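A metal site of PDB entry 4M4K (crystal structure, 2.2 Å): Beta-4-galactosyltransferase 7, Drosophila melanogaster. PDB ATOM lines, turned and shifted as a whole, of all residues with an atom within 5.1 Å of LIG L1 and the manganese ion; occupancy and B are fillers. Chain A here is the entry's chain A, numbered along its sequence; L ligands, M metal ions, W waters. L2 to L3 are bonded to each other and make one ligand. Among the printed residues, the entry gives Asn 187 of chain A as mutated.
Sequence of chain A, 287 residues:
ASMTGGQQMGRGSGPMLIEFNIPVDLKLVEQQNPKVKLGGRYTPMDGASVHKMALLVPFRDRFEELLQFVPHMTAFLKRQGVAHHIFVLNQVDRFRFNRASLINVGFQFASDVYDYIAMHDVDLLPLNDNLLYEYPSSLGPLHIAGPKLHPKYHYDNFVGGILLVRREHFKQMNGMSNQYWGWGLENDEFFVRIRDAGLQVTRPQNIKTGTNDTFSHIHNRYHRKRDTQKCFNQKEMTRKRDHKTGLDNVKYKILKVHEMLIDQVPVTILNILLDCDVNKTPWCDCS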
ATOM      1  N   VAL A  57      35.598  12.792  -9.848  1.00  0.00           N
ATOM      2  CA  VAL A  57      35.109  13.425 -11.061  1.00  0.00           C
ATOM      3  C   VAL A  57      35.300  12.532 -12.273  1.00  0.00           C
ATOM      4  O   VAL A  57      36.342  12.574 -12.929  1.00  0.00           O
ATOM      5  CB  VAL A  57      35.851  14.722 -11.339  1.00  0.00           C
ATOM      6  CG1 VAL A  57      35.221  15.439 -12.530  1.00  0.00           C
ATOM      7  CG2 VAL A  57      35.809  15.622 -10.099  1.00  0.00           C
ATOM      8  N   PRO A  58      34.293  11.700 -12.559  1.00  0.00           N
ATOM      9  CA  PRO A  58      34.296  10.910 -13.802  1.00  0.00           C
ATOM     10  C   PRO A  58      34.523  11.860 -14.955  1.00  0.00           C
ATOM     11  O   PRO A  58      33.903  12.918 -15.008  1.00  0.00           O
ATOM     12  CB  PRO A  58      32.865  10.374 -13.877  1.00  0.00           C
ATOM     13  CG  PRO A  58      32.398  10.338 -12.451  1.00  0.00           C
ATOM     14  CD  PRO A  58      33.074  11.512 -11.766  1.00  0.00           C
ATOM     15  N   PHE A  59      35.425  11.498 -15.869  1.00  0.00           N
ATOM     16  CA  PHE A  59      35.927  12.472 -16.798  1.00  0.00           C
ATOM     17  C   PHE A  59      36.321  11.863 -18.139  1.00  0.00           C
ATOM     18  O   PHE A  59      36.991  10.823 -18.179  1.00  0.00           O
ATOM     19  CB  PHE A  59      37.145  13.138 -16.161  1.00  0.00           C
ATOM     20  CG  PHE A  59      37.712  14.264 -16.964  1.00  0.00           C
ATOM     21  CD1 PHE A  59      37.246  15.555 -16.783  1.00  0.00           C
ATOM     22  CD2 PHE A  59      38.710  14.046 -17.897  1.00  0.00           C
ATOM     23  CE1 PHE A  59      37.766  16.614 -17.519  1.00  0.00           C
ATOM     24  CE2 PHE A  59      39.234  15.078 -18.628  1.00  0.00           C
ATOM     25  CZ  PHE A  59      38.772  16.377 -18.443  1.00  0.00           C
ATOM     26  N   ARG A  60      35.883  12.502 -19.222  1.00  0.00           N
ATOM     27  CA  ARG A  60      36.504  12.285 -20.533  1.00  0.00           C
ATOM     28  C   ARG A  60      36.259  13.500 -21.409  1.00  0.00           C
ATOM     29  O   ARG A  60      35.116  13.915 -21.597  1.00  0.00           O
ATOM     30  CB  ARG A  60      35.971  11.031 -21.223  1.00  0.00           C
ATOM     31  CG  ARG A  60      36.515  10.879 -22.664  1.00  0.00           C
ATOM     32  CD  ARG A  60      35.721   9.873 -23.437  1.00  0.00           C
ATOM     33  NE  ARG A  60      36.146   8.521 -23.130  1.00  0.00           N
ATOM     34  CZ  ARG A  60      35.393   7.440 -23.296  1.00  0.00           C
ATOM     35  NH1 ARG A  60      34.138   7.557 -23.745  1.00  0.00           N
ATOM     36  NH2 ARG A  60      35.887   6.241 -23.007  1.00  0.00           N
ATOM     37  N   ARG A  62      36.708  16.815 -21.223  1.00  0.00           N
ATOM     38  CA  ARG A  62      36.008  17.971 -20.657  1.00  0.00           C
ATOM     39  C   ARG A  62      37.047  18.896 -20.044  1.00  0.00           C
ATOM     40  O   ARG A  62      36.935  19.329 -18.895  1.00  0.00           O
ATOM     41  CB  ARG A  62      34.983  17.545 -19.603  1.00  0.00           C
ATOM     42  CG  ARG A  62      33.880  16.643 -20.124  1.00  0.00           C
ATOM     43  CD  ARG A  62      32.997  17.365 -21.131  1.00  0.00           C
ATOM     44  NE  ARG A  62      31.867  16.541 -21.566  1.00  0.00           N
ATOM     45  CZ  ARG A  62      31.844  15.829 -22.691  1.00  0.00           C
ATOM     46  NH1 ARG A  62      32.886  15.845 -23.509  1.00  0.00           N
ATOM     47  NH2 ARG A  62      30.763  15.119 -23.002  1.00  0.00           N
ATOM     48  N   PHE A  97      31.039   6.283 -22.465  1.00  0.00           N
ATOM     49  CA  PHE A  97      31.318   6.820 -21.147  1.00  0.00           C
ATOM     50  C   PHE A  97      30.567   6.106 -20.037  1.00  0.00           C
ATOM     51  O   PHE A  97      29.334   5.999 -20.058  1.00  0.00           O
ATOM     52  CB  PHE A  97      31.040   8.324 -21.107  1.00  0.00           C
ATOM     53  CG  PHE A  97      31.569   8.997 -19.889  1.00  0.00           C
ATOM     54  CD1 PHE A  97      32.932   9.189 -19.730  1.00  0.00           C
ATOM     55  CD2 PHE A  97      30.706   9.434 -18.889  1.00  0.00           C
ATOM     56  CE1 PHE A  97      33.428   9.827 -18.590  1.00  0.00           C
ATOM     57  CE2 PHE A  97      31.194  10.068 -17.760  1.00  0.00           C
ATOM     58  CZ  PHE A  97      32.564  10.259 -17.607  1.00  0.00           C
ATOM     59  N   ARG A  99      30.156   6.515 -16.306  1.00  0.00           N
ATOM     60  CA  ARG A  99      30.332   7.337 -15.121  1.00  0.00           C
ATOM     61  C   ARG A  99      30.399   6.503 -13.844  1.00  0.00           C
ATOM     62  O   ARG A  99      31.276   6.685 -12.988  1.00  0.00           O
ATOM     63  CB  ARG A  99      29.150   8.318 -15.043  1.00  0.00           C
ATOM     64  CG  ARG A  99      29.168   9.221 -13.839  1.00  0.00           C
ATOM     65  CD  ARG A  99      27.793   9.838 -13.563  1.00  0.00           C
ATOM     66  NE  ARG A  99      27.913  10.792 -12.472  1.00  0.00           N
ATOM     67  CZ  ARG A  99      27.132  10.840 -11.402  1.00  0.00           C
ATOM     68  NH1 ARG A  99      26.133   9.976 -11.236  1.00  0.00           N
ATOM     69  NH2 ARG A  99      27.367  11.771 -10.481  1.00  0.00           N
ATOM     70  N   HIS A 120      30.849  13.755  -8.474  1.00  0.00           N
ATOM     71  CA  HIS A 120      30.648  15.143  -8.893  1.00  0.00           C
ATOM     72  C   HIS A 120      30.777  15.346 -10.412  1.00  0.00           C
ATOM     73  O   HIS A 120      31.830  15.087 -10.973  1.00  0.00           O
ATOM     74  CB  HIS A 120      31.702  16.024  -8.219  1.00  0.00           C
ATOM     75  CG  HIS A 120      31.223  17.404  -7.877  1.00  0.00           C
ATOM     76  ND1 HIS A 120      30.748  18.282  -8.830  1.00  0.00           N
ATOM     77  CD2 HIS A 120      31.152  18.048  -6.690  1.00  0.00           C
ATOM     78  CE1 HIS A 120      30.400  19.419  -8.236  1.00  0.00           C
ATOM     79  NE2 HIS A 120      30.633  19.296  -6.933  1.00  0.00           N
ATOM     80  N   ASP A 121      29.716  15.827 -11.059  1.00  0.00           N
ATOM     81  CA  ASP A 121      29.830  16.268 -12.437  1.00  0.00           C
ATOM     82  C   ASP A 121      30.834  17.409 -12.576  1.00  0.00           C
ATOM     83  O   ASP A 121      30.912  18.276 -11.705  1.00  0.00           O
ATOM     84  CB  ASP A 121      28.481  16.727 -12.968  1.00  0.00           C
ATOM     85  CG  ASP A 121      27.450  15.625 -12.978  1.00  0.00           C
ATOM     86  OD1 ASP A 121      27.786  14.449 -12.669  1.00  0.00           O
ATOM     87  OD2 ASP A 121      26.291  15.935 -13.313  1.00  0.00           O
ATOM     88  N   VAL A 122      31.604  17.430 -13.660  1.00  0.00           N
ATOM     89  CA  VAL A 122      32.669  18.420 -13.832  1.00  0.00           C
ATOM     90  C   VAL A 122      32.114  19.797 -14.237  1.00  0.00           C
ATOM     91  O   VAL A 122      32.807  20.808 -14.119  1.00  0.00           O
ATOM     92  CB  VAL A 122      33.703  17.938 -14.866  1.00  0.00           C
ATOM     93  CG1 VAL A 122      33.137  18.096 -16.280  1.00  0.00           C
ATOM     94  CG2 VAL A 122      35.031  18.689 -14.731  1.00  0.00           C
ATOM     95  N   ASP A 123      30.859  19.839 -14.698  1.00  0.00           N
ATOM     96  CA  ASP A 123      30.266  21.042 -15.286  1.00  0.00           C
ATOM     97  C   ASP A 123      29.227  21.690 -14.366  1.00  0.00           C
ATOM     98  O   ASP A 123      28.476  22.582 -14.777  1.00  0.00           O
ATOM     99  CB  ASP A 123      29.590  20.710 -16.615  1.00  0.00           C
ATOM    100  CG  ASP A 123      28.492  19.660 -16.462  1.00  0.00           C
ATOM    101  OD1 ASP A 123      28.208  19.247 -15.313  1.00  0.00           O
ATOM    102  OD2 ASP A 123      27.907  19.248 -17.498  1.00  0.00           O
ATOM    103  N   LEU A 124      29.171  21.215 -13.129  1.00  0.00           N
ATOM    104  CA  LEU A 124      28.112  21.621 -12.195  1.00  0.00           C
ATOM    105  C   LEU A 124      28.725  22.256 -10.943  1.00  0.00           C
ATOM    106  O   LEU A 124      29.371  21.566 -10.136  1.00  0.00           O
ATOM    107  CB  LEU A 124      27.238  20.411 -11.854  1.00  0.00           C
ATOM    108  CG  LEU A 124      25.874  20.649 -11.185  1.00  0.00           C
ATOM    109  CD1 LEU A 124      24.986  21.501 -12.084  1.00  0.00           C
ATOM    110  CD2 LEU A 124      25.209  19.297 -10.880  1.00  0.00           C
ATOM    111  N   HIS A 150      18.358  22.045  -8.693  1.00  0.00           N
ATOM    112  CA  HIS A 150      19.020  21.776  -9.973  1.00  0.00           C
ATOM    113  C   HIS A 150      18.299  22.494 -11.130  1.00  0.00           C
ATOM    114  O   HIS A 150      17.067  22.488 -11.196  1.00  0.00           O
ATOM    115  CB  HIS A 150      19.100  20.270 -10.228  1.00  0.00           C
ATOM    116  CG  HIS A 150      20.057  19.885 -11.304  1.00  0.00           C
ATOM    117  ND1 HIS A 150      19.760  20.005 -12.646  1.00  0.00           N
ATOM    118  CD2 HIS A 150      21.322  19.405 -11.246  1.00  0.00           C
ATOM    119  CE1 HIS A 150      20.787  19.615 -13.366  1.00  0.00           C
ATOM    120  NE2 HIS A 150      21.760  19.244 -12.537  1.00  0.00           N
ATOM    121  N   TYR A 153      16.995  19.070 -13.713  1.00  0.00           N
ATOM    122  CA  TYR A 153      16.361  17.823 -13.274  1.00  0.00           C
ATOM    123  C   TYR A 153      15.608  17.999 -11.985  1.00  0.00           C
ATOM    124  O   TYR A 153      16.199  18.366 -10.958  1.00  0.00           O
ATOM    125  CB  TYR A 153      17.423  16.721 -13.138  1.00  0.00           C
ATOM    126  CG  TYR A 153      18.173  16.500 -14.429  1.00  0.00           C
ATOM    127  CD1 TYR A 153      17.499  16.143 -15.591  1.00  0.00           C
ATOM    128  CD2 TYR A 153      19.556  16.622 -14.482  1.00  0.00           C
ATOM    129  CE1 TYR A 153      18.176  15.923 -16.784  1.00  0.00           C
ATOM    130  CE2 TYR A 153      20.246  16.415 -15.661  1.00  0.00           C
ATOM    131  CZ  TYR A 153      19.550  16.058 -16.803  1.00  0.00           C
ATOM    132  OH  TYR A 153      20.236  15.859 -17.972  1.00  0.00           O
ATOM    133  N   PHE A 158      15.675  12.255  -8.047  1.00  0.00           N
ATOM    134  CA  PHE A 158      16.907  12.618  -8.744  1.00  0.00           C
ATOM    135  C   PHE A 158      18.029  12.714  -7.708  1.00  0.00           C
ATOM    136  O   PHE A 158      17.924  13.482  -6.751  1.00  0.00           O
ATOM    137  CB  PHE A 158      16.757  13.948  -9.490  1.00  0.00           C
ATOM    138  CG  PHE A 158      18.052  14.493 -10.019  1.00  0.00           C
ATOM    139  CD1 PHE A 158      18.677  13.910 -11.125  1.00  0.00           C
ATOM    140  CD2 PHE A 158      18.652  15.599  -9.430  1.00  0.00           C
ATOM    141  CE1 PHE A 158      19.878  14.411 -11.622  1.00  0.00           C
ATOM    142  CE2 PHE A 158      19.844  16.113  -9.923  1.00  0.00           C
ATOM    143  CZ  PHE A 158      20.463  15.517 -11.019  1.00  0.00           C
ATOM    144  N   GLY A 160      21.358  12.766  -9.042  1.00  0.00           N
ATOM    145  CA  GLY A 160      22.498  12.971  -9.907  1.00  0.00           C
ATOM    146  C   GLY A 160      23.277  14.238  -9.600  1.00  0.00           C
ATOM    147  O   GLY A 160      22.999  14.934  -8.608  1.00  0.00           O
ATOM    148  N   GLY A 161      24.272  14.535 -10.432  1.00  0.00           N
ATOM    149  CA  GLY A 161      25.018  15.772 -10.323  1.00  0.00           C
ATOM    150  C   GLY A 161      26.038  15.782  -9.202  1.00  0.00           C
ATOM    151  O   GLY A 161      27.246  15.712  -9.455  1.00  0.00           O
ATOM    152  N   GLY A 182      27.249   4.814 -21.532  1.00  0.00           N
ATOM    153  CA  GLY A 182      26.539   5.901 -22.169  1.00  0.00           C
ATOM    154  C   GLY A 182      25.658   6.629 -21.154  1.00  0.00           C
ATOM    155  O   GLY A 182      25.495   6.160 -20.020  1.00  0.00           O
ATOM    156  N   TRP A 183      25.080   7.744 -21.576  1.00  0.00           N
ATOM    157  CA  TRP A 183      24.319   8.609 -20.700  1.00  0.00           C
ATOM    158  C   TRP A 183      23.120   7.931 -20.034  1.00  0.00           C
ATOM    159  O   TRP A 183      22.393   7.140 -20.666  1.00  0.00           O
ATOM    160  CB  TRP A 183      23.829   9.818 -21.487  1.00  0.00           C
ATOM    161  CG  TRP A 183      23.041  10.830 -20.658  1.00  0.00           C
ATOM    162  CD1 TRP A 183      23.537  11.960 -20.050  1.00  0.00           C
ATOM    163  CD2 TRP A 183      21.634  10.817 -20.370  1.00  0.00           C
ATOM    164  NE1 TRP A 183      22.533  12.638 -19.402  1.00  0.00           N
ATOM    165  CE2 TRP A 183      21.355  11.960 -19.583  1.00  0.00           C
ATOM    166  CE3 TRP A 183      20.584   9.940 -20.700  1.00  0.00           C
ATOM    167  CZ2 TRP A 183      20.064  12.242 -19.117  1.00  0.00           C
ATOM    168  CZ3 TRP A 183      19.298  10.235 -20.244  1.00  0.00           C
ATOM    169  CH2 TRP A 183      19.049  11.377 -19.455  1.00  0.00           C
ATOM    170  N   GLY A 184      22.929   8.234 -18.745  1.00  0.00           N
ATOM    171  CA  GLY A 184      21.650   8.042 -18.105  1.00  0.00           C
ATOM    172  C   GLY A 184      21.450   6.819 -17.240  1.00  0.00           C
ATOM    173  O   GLY A 184      22.118   5.785 -17.430  1.00  0.00           O
ATOM    174  N   LEU A 185      20.520   6.978 -16.290  1.00  0.00           N
ATOM    175  CA  LEU A 185      19.973   5.917 -15.437  1.00  0.00           C
ATOM    176  C   LEU A 185      20.865   5.436 -14.294  1.00  0.00           C
ATOM    177  O   LEU A 185      20.351   4.900 -13.317  1.00  0.00           O
ATOM    178  CB  LEU A 185      19.470   4.729 -16.258  1.00  0.00           C
ATOM    179  CG  LEU A 185      18.258   5.005 -17.152  1.00  0.00           C
ATOM    180  CD1 LEU A 185      17.953   3.760 -17.978  1.00  0.00           C
ATOM    181  CD2 LEU A 185      17.034   5.424 -16.308  1.00  0.00           C
ATOM    182  N   GLU A 186      22.179   5.635 -14.381  1.00  0.00           N
ATOM    183  CA  GLU A 186      23.084   5.065 -13.368  1.00  0.00           C
ATOM    184  C   GLU A 186      22.762   5.581 -11.962  1.00  0.00           C
ATOM    185  O   GLU A 186      22.747   4.810 -10.998  1.00  0.00           O
ATOM    186  CB  GLU A 186      24.573   5.247 -13.751  1.00  0.00           C
ATOM    187  CG  GLU A 186      25.228   6.557 -13.314  1.00  0.00           C
ATOM    188  CD  GLU A 186      24.617   7.795 -13.968  1.00  0.00           C
ATOM    189  OE1 GLU A 186      24.120   7.687 -15.123  1.00  0.00           O
ATOM    190  OE2 GLU A 186      24.620   8.873 -13.331  1.00  0.00           O
ATOM    191  N   ASN A 187      22.461   6.869 -11.853  1.00  0.00           N
ATOM    192  CA  ASN A 187      22.082   7.462 -10.570  1.00  0.00           C
ATOM    193  C   ASN A 187      20.716   7.007 -10.076  1.00  0.00           C
ATOM    194  O   ASN A 187      20.484   6.930  -8.865  1.00  0.00           O
ATOM    195  CB  ASN A 187      22.084   8.990 -10.670  1.00  0.00           C
ATOM    196  CG  ASN A 187      21.302   9.502 -11.856  1.00  0.00           C
ATOM    197  OD1 ASN A 187      21.362   8.918 -12.955  1.00  0.00           O
ATOM    198  ND2 ASN A 187      20.567  10.598 -11.666  1.00  0.00           N
ATOM    199  N   HIS A 217      25.240  25.278 -14.483  1.00  0.00           N
ATOM    200  CA  HIS A 217      25.408  24.070 -15.284  1.00  0.00           C
ATOM    201  C   HIS A 217      25.802  24.508 -16.683  1.00  0.00           C
ATOM    202  O   HIS A 217      24.967  24.564 -17.590  1.00  0.00           O
ATOM    203  CB  HIS A 217      24.104  23.279 -15.347  1.00  0.00           C
ATOM    204  CG  HIS A 217      24.227  21.953 -16.046  1.00  0.00           C
ATOM    205  ND1 HIS A 217      23.174  21.335 -16.683  1.00  0.00           N
ATOM    206  CD2 HIS A 217      25.293  21.127 -16.210  1.00  0.00           C
ATOM    207  CE1 HIS A 217      23.575  20.192 -17.204  1.00  0.00           C
ATOM    208  NE2 HIS A 217      24.865  20.043 -16.938  1.00  0.00           N
ATOM    209  N   HIS A 219      26.724  23.651 -19.745  1.00  0.00           N
ATOM    210  CA  HIS A 219      26.662  22.440 -20.560  1.00  0.00           C
ATOM    211  C   HIS A 219      25.753  22.695 -21.759  1.00  0.00           C
ATOM    212  O   HIS A 219      24.527  22.561 -21.667  1.00  0.00           O
ATOM    213  CB  HIS A 219      26.116  21.271 -19.732  1.00  0.00           C
ATOM    214  CG  HIS A 219      26.141  19.948 -20.448  1.00  0.00           C
ATOM    215  ND1 HIS A 219      26.042  18.744 -19.784  1.00  0.00           N
ATOM    216  CD2 HIS A 219      26.241  19.647 -21.763  1.00  0.00           C
ATOM    217  CE1 HIS A 219      26.084  17.757 -20.655  1.00  0.00           C
ATOM    218  NE2 HIS A 219      26.210  18.272 -21.860  1.00  0.00           N
ATOM    219  N   ARG A 226      25.021  14.379 -25.265  1.00  0.00           N
ATOM    220  CA  ARG A 226      24.720  13.266 -24.394  1.00  0.00           C
ATOM    221  C   ARG A 226      24.633  11.994 -25.234  1.00  0.00           C
ATOM    222  O   ARG A 226      23.896  11.921 -26.208  1.00  0.00           O
ATOM    223  CB  ARG A 226      23.408  13.510 -23.626  1.00  0.00           C
ATOM    224  CG  ARG A 226      23.480  14.696 -22.653  1.00  0.00           C
ATOM    225  CD  ARG A 226      22.158  14.937 -21.894  1.00  0.00           C
ATOM    226  NE  ARG A 226      22.369  15.891 -20.809  1.00  0.00           N
ATOM    227  CZ  ARG A 226      22.396  17.218 -20.950  1.00  0.00           C
ATOM    228  NH1 ARG A 226      22.186  17.770 -22.136  1.00  0.00           N
ATOM    229  NH2 ARG A 226      22.615  18.006 -19.894  1.00  0.00           N
HETATM  230  N1  LIG L   1      31.261  13.298 -18.487  1.00  0.00           N
HETATM  231  C1  LIG L   1      32.440  13.376 -19.143  1.00  0.00           C
HETATM  232  N2  LIG L   1      32.563  13.037 -20.416  1.00  0.00           N
HETATM  233  C2  LIG L   1      31.501  12.574 -21.111  1.00  0.00           C
HETATM  234  C3  LIG L   1      30.247  12.460 -20.461  1.00  0.00           C
HETATM  235  C4  LIG L   1      30.170  12.852 -19.110  1.00  0.00           C
HETATM  236  O1  LIG L   1      33.416  13.785 -18.540  1.00  0.00           O
HETATM  237  O2  LIG L   1      31.609  12.202 -22.458  1.00  0.00           O
HETATM  238  C5  LIG L   1      31.191  13.631 -17.141  1.00  0.00           C
HETATM  239  C6  LIG L   1      31.152  15.118 -16.798  1.00  0.00           C
HETATM  240  O3  LIG L   1      31.721  15.226 -15.520  1.00  0.00           O
HETATM  241  C7  LIG L   1      29.721  15.390 -16.778  1.00  0.00           C
HETATM  242  C8  LIG L   1      29.233  14.216 -16.021  1.00  0.00           C
HETATM  243  O4  LIG L   1      29.983  13.086 -16.533  1.00  0.00           O
HETATM  244  O5  LIG L   1      29.400  16.627 -16.144  1.00  0.00           O
HETATM  245  C9  LIG L   1      27.755  13.971 -16.244  1.00  0.00           C
HETATM  246  O6  LIG L   1      27.539  13.841 -17.624  1.00  0.00           O
HETATM  247  P1  LIG L   1      26.660  14.935 -18.416  1.00  0.00           P
HETATM  248  O7  LIG L   1      26.961  16.363 -17.910  1.00  0.00           O
HETATM  249  O8  LIG L   1      27.008  14.827 -19.880  1.00  0.00           O
HETATM  250  O9  LIG L   1      25.086  14.608 -18.211  1.00  0.00           O
HETATM  251  P2  LIG L   1      24.007  15.512 -17.473  1.00  0.00           P
HETATM  252  O10 LIG L   1      24.322  17.024 -17.647  1.00  0.00           O
HETATM  253  O11 LIG L   1      22.652  15.202 -18.077  1.00  0.00           O
HETATM  254  O12 LIG L   1      24.018  15.158 -15.902  1.00  0.00           O
HETATM  255  C10 LIG L   1      23.102  14.242 -15.306  1.00  0.00           C
HETATM  256  C11 LIG L   1      23.588  13.967 -13.975  1.00  0.00           C
HETATM  257  C12 LIG L   1      24.778  13.160 -14.034  1.00  0.00           C
HETATM  258  C13 LIG L   1      24.490  11.822 -14.573  1.00  0.00           C
HETATM  259  C14 LIG L   1      24.038  11.909 -16.098  1.00  0.00           C
HETATM  260  C15 LIG L   1      23.498  10.737 -16.561  1.00  0.00           C
HETATM  261  O13 LIG L   1      23.923  15.320 -13.326  1.00  0.00           O
HETATM  262  O14 LIG L   1      25.414  13.068 -12.678  1.00  0.00           O
HETATM  263  O15 LIG L   1      23.449  11.241 -13.768  1.00  0.00           O
HETATM  264  O16 LIG L   1      22.988  13.059 -16.192  1.00  0.00           O
HETATM  265  O17 LIG L   1      24.435   9.882 -16.835  1.00  0.00           O
HETATM  266  O1  LG2 L   2      11.144  12.157 -17.321  1.00  0.00           O
HETATM  267  C1  LG2 L   2      12.475  11.747 -17.549  1.00  0.00           C
HETATM  268  C2  LG2 L   2      13.381  12.944 -17.397  1.00  0.00           C
HETATM  269  C3  LG2 L   2      14.786  12.529 -17.603  1.00  0.00           C
HETATM  270  C4  LG2 L   2      15.166  11.508 -16.631  1.00  0.00           C
HETATM  271  C5  LG2 L   2      14.263  10.311 -16.706  1.00  0.00           C
HETATM  272  O2  LG2 L   2      13.018  13.951 -18.380  1.00  0.00           O
HETATM  273  O3  LG2 L   2      15.675  13.642 -17.424  1.00  0.00           O
HETATM  274  O4  LG2 L   2      16.512  11.107 -17.006  1.00  0.00           O
HETATM  275  O5  LG2 L   2      12.829  10.684 -16.619  1.00  0.00           O
HETATM  276  C1  LG3 L   3      17.361  11.263 -15.927  1.00  0.00           C
HETATM  277  C2  LG3 L   3      18.510  10.266 -16.099  1.00  0.00           C
HETATM  278  C3  LG3 L   3      19.497  10.459 -15.020  1.00  0.00           C
HETATM  279  C4  LG3 L   3      20.028  11.834 -15.029  1.00  0.00           C
HETATM  280  C5  LG3 L   3      18.888  12.878 -14.922  1.00  0.00           C
HETATM  281  O1  LG3 L   3      17.965   8.932 -16.091  1.00  0.00           O
HETATM  282  O2  LG3 L   3      20.573   9.506 -15.169  1.00  0.00           O
HETATM  283  O3  LG3 L   3      20.920  12.054 -13.922  1.00  0.00           O
HETATM  284  O4  LG3 L   3      17.826  12.642 -15.905  1.00  0.00           O
HETATM  285 MN    MN M   1      25.985  18.265 -17.517  1.00  0.00          MN
HETATM  286  O   HOH W   1      25.557   6.596 -17.147  1.00  0.00           O
HETATM  287  O   HOH W   2      23.556  18.041 -14.347  1.00  0.00           O
HETATM  288  O   HOH W   3      26.188  17.897 -15.192  1.00  0.00           O
HETATM  289  O   HOH W   4      27.102  10.219 -17.892  1.00  0.00           O
HETATM  290  O   HOH W   5      29.424  16.399 -20.227  1.00  0.00           O
HETATM  291  O   HOH W   6      27.928  15.105 -22.490  1.00  0.00           O
HETATM  292  O   HOH W   7      27.083  11.934 -19.982  1.00  0.00           O
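The side-chain carboxylate (OE2) of Glu 186 lies within hydrogen-bond range of an oxygen (O15) of LIG L1 (2.7 Å).
An oxygen (O1) of LIG L1 sits at hydrogen-bond distance from the backbone NH (N) of Arg 60 (2.9 Å).
An oxygen (O11) of LIG L1 lies within hydrogen-bond range of the side-chain hydroxyl (OH) of Tyr 153 (2.5 Å).
N of Gly 184 sits at hydrogen-bond distance from O17 of LIG L1, at 2.9 Å.
O14 of LIG L1 lies close to NH2 of Arg 99.
A nitrogen (N2) of LIG L1 is in hydrogen-bond range of the backbone carbonyl oxygen (O) of Arg 60 (2.9 Å).
An oxygen (O11) of LIG L1 lies within hydrogen-bond range of the indole nitrogen (NE1) of Trp 183, at 2.9 Å.
An oxygen (O13) of LIG L1 is in hydrogen-bond range of the side-chain carboxylate (OD2) of Asp 121 (2.4 Å).
An oxygen (O15) of LIG L1 sits at hydrogen-bond distance from the side-chain amide oxygen (OD1) of Asn 187 (3.2 Å).
The guanidinium group of Arg 226 is in salt-bridge range of an oxygen (O11) of LIG L1, 2.8 Å away.
An oxygen (O14) of LIG L1 is in hydrogen-bond range of the backbone NH of Gly 161 (2.9 Å).
N of Leu 185 sits at hydrogen-bond distance from O2 of LG3 L3 (2.8 Å).
The guanidinium group of Arg 62 sits at hydrogen-bond distance from an oxygen (O2) of LIG L1, at 3.1 Å.
N of Val 122 lies within hydrogen-bond range of O3 of LIG L1.
OD1 of Asn 187 is in hydrogen-bond range of O2 of LG3 L3.
O3 of LIG L1 lies within hydrogen-bond range of O of Pro 58 (3.2 Å).
O15 of LIG L1 is in hydrogen-bond range of O3 of LG3 L3, at 2.7 Å.
The side-chain amide oxygen (OD1) of Asn 187 sits close to the side-chain carboxylate (OE2) of Glu 186 (3.3 Å).
The backbone carbonyl oxygen of Phe 97 sits at hydrogen-bond distance from the backbone NH of Gly 182 (2.8 Å).
The backbone carbonyl oxygen of Gly 161 is in hydrogen-bond range of the backbone NH of Asp 121, at 2.9 Å.
The backbone NH of Tyr 153 lies within hydrogen-bond range of a ring nitrogen (ND1) of His 150 (3.1 Å).
The side-chain amide nitrogen (ND2) of Asn 187 sits close to the backbone NH (N) of Gly 160 (3.5 Å).
OD1 of Asp 121 lies within salt-bridge range of NH2 of Arg 99, at 3.5 Å.
The side-chain carboxylate (OE2) of Glu 186 lies within salt-bridge range of the guanidinium group (NH1) of Arg 99 (2.8 Å).
Phe 59 touches LIG L1.
Phe 97 touches LIG L1 (CE2 to C4, 3.3 Å).
Gly 160 touches LIG L1 (C to O14, 3.9 Å).
Of the 26 residues printed, 3 come within 4 Å of the manganese ion.
The nearest printed residue that does not touch the manganese ion is Arg 226 (4.1 Å).
The manganese ion is bound by O10 of LIG L1 (2.1 Å), OD2 of Asp 123 (2.2 Å), O7 of LIG L1 (2.2 Å), NE2 of His 217 (2.2 Å), ND1 of His 219 (2.3 Å) and water W3 (2.4 Å).
The manganese ion has six donor atoms within binding distance.
Water W3 lies within hydrogen-bond range of the side-chain carboxylate (OD1) of Asp 123 and the side-chain carboxylate (OD2) of Asp 121.
Water W6 bridges O8 of LIG L1 (2.8 Å) and NH2 of Arg 62 (2.9 Å).
Water W5 bridges NE of Arg 62 (2.8 Å) and O8 of LIG L1 (2.9 Å).
Water W2 bridges a ring nitrogen (NE2) of His 150 (2.8 Å) and an oxygen (O13) of LIG L1 (2.9 Å).
Water W1 lies within hydrogen-bond range of the side-chain carboxylate of Glu 186 (2.7 Å), the backbone carbonyl oxygen of Gly 182 (2.9 Å), the backbone NH of Gly 184 (3.5 Å) and an oxygen (O17) of LIG L1 (3.5 Å).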
